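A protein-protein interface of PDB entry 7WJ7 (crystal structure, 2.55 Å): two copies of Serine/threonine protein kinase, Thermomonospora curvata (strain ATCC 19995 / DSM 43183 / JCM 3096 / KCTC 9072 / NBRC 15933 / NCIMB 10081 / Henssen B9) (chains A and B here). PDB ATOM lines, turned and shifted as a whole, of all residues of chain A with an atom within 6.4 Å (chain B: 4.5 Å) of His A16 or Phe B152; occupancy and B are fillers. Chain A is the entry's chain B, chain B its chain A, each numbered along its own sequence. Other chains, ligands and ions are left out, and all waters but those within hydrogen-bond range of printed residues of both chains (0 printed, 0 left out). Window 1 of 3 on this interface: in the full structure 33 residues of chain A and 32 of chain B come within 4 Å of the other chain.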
ATOM      1  N   ALA A  14      24.059  -2.119  29.351  1.00  0.00           N
ATOM      2  CA  ALA A  14      23.664  -0.785  28.911  1.00  0.00           C
ATOM      3  C   ALA A  14      23.618  -0.779  27.389  1.00  0.00           C
ATOM      4  O   ALA A  14      24.662  -0.817  26.730  1.00  0.00           O
ATOM      5  CB  ALA A  14      24.630   0.275  29.436  1.00  0.00           C
ATOM      6  N   LEU A  15      22.408  -0.720  26.833  1.00  0.00           N
ATOM      7  CA  LEU A  15      22.225  -0.823  25.391  1.00  0.00           C
ATOM      8  C   LEU A  15      22.304   0.530  24.690  1.00  0.00           C
ATOM      9  O   LEU A  15      23.043   0.679  23.713  1.00  0.00           O
ATOM     10  CB  LEU A  15      20.885  -1.499  25.082  1.00  0.00           C
ATOM     11  CG  LEU A  15      20.627  -2.826  25.794  1.00  0.00           C
ATOM     12  CD1 LEU A  15      19.251  -3.367  25.436  1.00  0.00           C
ATOM     13  CD2 LEU A  15      21.710  -3.836  25.449  1.00  0.00           C
ATOM     14  N   HIS A  16      21.552   1.521  25.166  1.00  0.00           N
ATOM     15  CA  HIS A  16      21.503   2.807  24.485  1.00  0.00           C
ATOM     16  C   HIS A  16      20.998   3.877  25.442  1.00  0.00           C
ATOM     17  O   HIS A  16      20.294   3.583  26.413  1.00  0.00           O
ATOM     18  CB  HIS A  16      20.608   2.749  23.241  1.00  0.00           C
ATOM     19  N   PHE A  17      21.365   5.122  25.144  1.00  0.00           N
ATOM     20  CA  PHE A  17      20.889   6.290  25.873  1.00  0.00           C
ATOM     21  C   PHE A  17      20.770   7.446  24.892  1.00  0.00           C
ATOM     22  O   PHE A  17      21.662   7.657  24.065  1.00  0.00           O
ATOM     23  CB  PHE A  17      21.832   6.659  27.024  1.00  0.00           C
ATOM     24  CG  PHE A  17      21.370   7.828  27.850  1.00  0.00           C
ATOM     25  CD1 PHE A  17      20.531   7.638  28.934  1.00  0.00           C
ATOM     26  CD2 PHE A  17      21.796   9.114  27.556  1.00  0.00           C
ATOM     27  CE1 PHE A  17      20.113   8.710  29.700  1.00  0.00           C
ATOM     28  CE2 PHE A  17      21.381  10.192  28.319  1.00  0.00           C
ATOM     29  CZ  PHE A  17      20.539   9.990  29.393  1.00  0.00           C
ATOM     30  N   SER A  18      19.666   8.188  24.986  1.00  0.00           N
ATOM     31  CA  SER A  18      19.419   9.300  24.077  1.00  0.00           C
ATOM     32  C   SER A  18      18.308  10.200  24.604  1.00  0.00           C
ATOM     33  O   SER A  18      17.216   9.719  24.926  1.00  0.00           O
ATOM     34  CB  SER A  18      19.057   8.780  22.683  1.00  0.00           C
ATOM     35  OG  SER A  18      19.498   9.674  21.678  1.00  0.00           O
ATOM     36  N   GLY A  21      16.771   9.505  27.964  1.00  0.00           N
ATOM     37  CA  GLY A  21      16.199   8.178  28.074  1.00  0.00           C
ATOM     38  C   GLY A  21      17.189   7.077  27.754  1.00  0.00           C
ATOM     39  O   GLY A  21      17.891   7.141  26.740  1.00  0.00           O
ATOM     40  N   GLY A  22      17.252   6.058  28.609  1.00  0.00           N
ATOM     41  CA  GLY A  22      18.161   4.947  28.403  1.00  0.00           C
ATOM     42  C   GLY A  22      17.457   3.615  28.240  1.00  0.00           C
ATOM     43  O   GLY A  22      16.316   3.452  28.680  1.00  0.00           O
ATOM     44  N   VAL A  23      18.124   2.656  27.605  1.00  0.00           N
ATOM     45  CA  VAL A  23      17.567   1.329  27.368  1.00  0.00           C
ATOM     46  C   VAL A  23      18.562   0.302  27.882  1.00  0.00           C
ATOM     47  O   VAL A  23      19.734   0.318  27.489  1.00  0.00           O
ATOM     48  CB  VAL A  23      17.263   1.091  25.877  1.00  0.00           C
ATOM     49  CG1 VAL A  23      16.802  -0.342  25.647  1.00  0.00           C
ATOM     50  CG2 VAL A  23      16.217   2.082  25.388  1.00  0.00           C
ATOM     51  N   TYR A  24      18.100  -0.588  28.756  1.00  0.00           N
ATOM     52  CA  TYR A  24      18.970  -1.556  29.401  1.00  0.00           C
ATOM     53  C   TYR A  24      18.377  -2.951  29.299  1.00  0.00           C
ATOM     54  O   TYR A  24      17.158  -3.126  29.218  1.00  0.00           O
ATOM     55  CB  TYR A  24      19.200  -1.204  30.874  1.00  0.00           C
ATOM     56  CG  TYR A  24      19.786   0.168  31.074  1.00  0.00           C
ATOM     57  CD1 TYR A  24      21.160   0.364  31.069  1.00  0.00           C
ATOM     58  CD2 TYR A  24      18.967   1.272  31.249  1.00  0.00           C
ATOM     59  CE1 TYR A  24      21.703   1.620  31.245  1.00  0.00           C
ATOM     60  CE2 TYR A  24      19.497   2.533  31.424  1.00  0.00           C
ATOM     61  CZ  TYR A  24      20.868   2.702  31.421  1.00  0.00           C
ATOM     62  OH  TYR A  24      21.409   3.955  31.596  1.00  0.00           O
ATOM     63  N   GLU A  39      14.021   3.713  30.859  1.00  0.00           N
ATOM     64  CA  GLU A  39      13.798   4.635  31.962  1.00  0.00           C
ATOM     65  C   GLU A  39      13.982   6.064  31.472  1.00  0.00           C
ATOM     66  O   GLU A  39      14.715   6.326  30.515  1.00  0.00           O
ATOM     67  CB  GLU A  39      14.734   4.338  33.144  1.00  0.00           C
ATOM     68  CG  GLU A  39      16.161   4.022  32.743  1.00  0.00           C
ATOM     69  CD  GLU A  39      16.959   5.269  32.437  1.00  0.00           C
ATOM     70  OE1 GLU A  39      16.799   6.269  33.171  1.00  0.00           O
ATOM     71  OE2 GLU A  39      17.741   5.253  31.464  1.00  0.00           O
ATOM     72  N   ASN B  99      30.303   1.979  27.573  1.00  0.00           N
ATOM     73  CA  ASN B  99      29.145   1.301  28.145  1.00  0.00           C
ATOM     74  C   ASN B  99      29.161  -0.204  27.901  1.00  0.00           C
ATOM     75  O   ASN B  99      28.484  -0.942  28.625  1.00  0.00           O
ATOM     76  CB  ASN B  99      27.854   1.908  27.590  1.00  0.00           C
ATOM     77  CG  ASN B  99      27.698   1.689  26.097  1.00  0.00           C
ATOM     78  OD1 ASN B  99      28.200   2.468  25.284  1.00  0.00           O
ATOM     79  ND2 ASN B  99      26.993   0.626  25.727  1.00  0.00           N
ATOM     80  N   HIS B 150      28.906  10.956  28.868  1.00  0.00           N
ATOM     81  CA  HIS B 150      28.493   9.779  29.620  1.00  0.00           C
ATOM     82  C   HIS B 150      29.085   8.560  28.922  1.00  0.00           C
ATOM     83  O   HIS B 150      29.751   8.677  27.888  1.00  0.00           O
ATOM     84  CB  HIS B 150      26.970   9.699  29.741  1.00  0.00           C
ATOM     85  CG  HIS B 150      26.243   9.863  28.443  1.00  0.00           C
ATOM     86  ND1 HIS B 150      26.340   8.955  27.410  1.00  0.00           N
ATOM     87  CD2 HIS B 150      25.395  10.828  28.015  1.00  0.00           C
ATOM     88  CE1 HIS B 150      25.588   9.356  26.401  1.00  0.00           C
ATOM     89  NE2 HIS B 150      25.004  10.491  26.741  1.00  0.00           N
ATOM     90  N   MET B 151      28.825   7.382  29.495  1.00  0.00           N
ATOM     91  CA  MET B 151      29.493   6.157  29.064  1.00  0.00           C
ATOM     92  C   MET B 151      29.162   5.760  27.630  1.00  0.00           C
ATOM     93  O   MET B 151      29.924   4.999  27.023  1.00  0.00           O
ATOM     94  CB  MET B 151      29.134   5.010  30.008  1.00  0.00           C
ATOM     95  CG  MET B 151      27.647   4.695  30.085  1.00  0.00           C
ATOM     96  SD  MET B 151      27.302   3.543  31.434  1.00  0.00           S
ATOM     97  CE  MET B 151      25.531   3.322  31.287  1.00  0.00           C
ATOM     98  N   PHE B 152      28.050   6.239  27.075  1.00  0.00           N
ATOM     99  CA  PHE B 152      27.691   5.878  25.709  1.00  0.00           C
ATOM    100  C   PHE B 152      28.435   6.699  24.668  1.00  0.00           C
ATOM    101  O   PHE B 152      28.484   6.295  23.500  1.00  0.00           O
ATOM    102  CB  PHE B 152      26.187   6.038  25.497  1.00  0.00           C
ATOM    103  CG  PHE B 152      25.362   5.130  26.349  1.00  0.00           C
ATOM    104  CD1 PHE B 152      25.011   3.865  25.903  1.00  0.00           C
ATOM    105  CD2 PHE B 152      24.961   5.530  27.613  1.00  0.00           C
ATOM    106  CE1 PHE B 152      24.253   3.022  26.698  1.00  0.00           C
ATOM    107  CE2 PHE B 152      24.204   4.693  28.413  1.00  0.00           C
ATOM    108  CZ  PHE B 152      23.849   3.439  27.955  1.00  0.00           C
ATOM    109  N   ASN B 153      29.011   7.833  25.059  1.00  0.00           N
ATOM    110  CA  ASN B 153      29.692   8.732  24.140  1.00  0.00           C
ATOM    111  C   ASN B 153      31.210   8.600  24.185  1.00  0.00           C
ATOM    112  O   ASN B 153      31.895   9.247  23.387  1.00  0.00           O
ATOM    113  CB  ASN B 153      29.298  10.188  24.437  1.00  0.00           C
ATOM    114  CG  ASN B 153      28.124  10.667  23.598  1.00  0.00           C
ATOM    115  OD1 ASN B 153      28.119  10.525  22.376  1.00  0.00           O
ATOM    116  ND2 ASN B 153      27.125  11.246  24.253  1.00  0.00           N
ATOM    117  N   ILE B 154      31.753   7.786  25.088  1.00  0.00           N
ATOM    118  CA  ILE B 154      33.196   7.654  25.265  1.00  0.00           C
ATOM    119  C   ILE B 154      33.667   6.381  24.578  1.00  0.00           C
ATOM    120  O   ILE B 154      33.155   5.289  24.854  1.00  0.00           O
ATOM    121  CB  ILE B 154      33.580   7.648  26.757  1.00  0.00           C
ATOM    122  CG1 ILE B 154      33.225   8.989  27.406  1.00  0.00           C
ATOM    123  CG2 ILE B 154      35.062   7.354  26.927  1.00  0.00           C
ATOM    124  CD1 ILE B 154      33.000   8.917  28.903  1.00  0.00           C
ATOM    125  N   ILE B 165      32.422  10.784  20.750  1.00  0.00           N
ATOM    126  CA  ILE B 165      31.856  10.221  19.535  1.00  0.00           C
ATOM    127  C   ILE B 165      30.780  11.108  18.917  1.00  0.00           C
ATOM    128  O   ILE B 165      30.753  11.286  17.695  1.00  0.00           O
ATOM    129  CB  ILE B 165      31.324   8.786  19.775  1.00  0.00           C
ATOM    130  CG1 ILE B 165      31.232   8.081  18.434  1.00  0.00           C
ATOM    131  CG2 ILE B 165      29.992   8.767  20.503  1.00  0.00           C
ATOM    132  CD1 ILE B 165      32.472   8.352  17.624  1.00  0.00           C
ATOM    133  N   PRO B 184      22.753   9.537  32.269  1.00  0.00           N
ATOM    134  CA  PRO B 184      22.248   8.191  32.485  1.00  0.00           C
ATOM    135  C   PRO B 184      22.143   7.762  33.954  1.00  0.00           C
ATOM    136  O   PRO B 184      21.279   6.982  34.255  1.00  0.00           O
ATOM    137  CB  PRO B 184      23.299   7.327  31.780  1.00  0.00           C
ATOM    138  CG  PRO B 184      23.805   8.187  30.668  1.00  0.00           C
ATOM    139  CD  PRO B 184      23.782   9.584  31.239  1.00  0.00           C
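The side-chain amide nitrogen of Asn B99 is in hydrogen-bond range of the backbone carbonyl oxygen of Ala A14, at 2.9 Å.
A ring nitrogen (NE2) of His B150 sits close to the side-chain amide nitrogen (ND2) of Asn B153 (3.4 Å). N of Phe B152 lies close to ND1 of His B150 (3.2 Å). The backbone carbonyl oxygen (O) of Val A23 lies within hydrogen-bond range of the backbone NH (N) of Leu A15 (2.9 Å). The backbone carbonyl oxygen (O) of Met B151 sits at hydrogen-bond distance from the backbone NH (N) of Asn B99 (3.1 Å). O of His A16 is in hydrogen-bond range of N of Val A23.
Ala A14 touches Met B151 (CB to CE, 3.7 Å). CZ of Phe B152 touches CB of Ala A14 (3.6 Å). Leu A15 touches Phe B152 (C to CE1, 3.7 Å). Phe B152 touches His A16 (CE1 to N, 3.4 Å). His B150 touches Phe A17 (NE2 to CD2, 3.6 Å). Phe A17 touches Phe B152 (CB to CD2, 3.4 Å). Phe A17 touches Pro B184. Pro B184 touches Tyr A24 (CB to OH, 3.9 Å).
Printed residues of chain B within 4 Å of Leu A15: Phe B152 (3.7 Å). His A16 touches just one residue of chain B: Phe B152 (3.4 Å). Printed residues of chain B within 4 Å of Tyr A24: Pro B184 (3.9 Å). Of the printed residues of chain A, Met B151 touches Ala A14. Of chain A, only Ala A14 (3.6 Å), Leu A15 (3.7 Å), His A16 (3.4 Å) and Phe A17 (3.4 Å) come within 4 Å of Phe B152. Of the printed residues of chain A, Pro B184 touches Phe A17 and Tyr A24. The nearest printed residue of chain B that does not touch His A16 is Asn B99 (5.5 Å). The nearest residue of chain A that does not touch Phe B152 is Tyr A24 (4.3 Å).
Of the 8 printed residues of chain B, 5 touch a printed residue of chain A. Printed residues of chain A that touch a printed residue of chain B: Ala A14, Leu A15, His A16, Phe A17 and Tyr A24. Among the printed residues, 9 pairs touch across the chains.
No position is printed for both chains. Of the 9 pairs that touch across the chains among the printed residues, none has its exchanged pair printed and touching as well.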
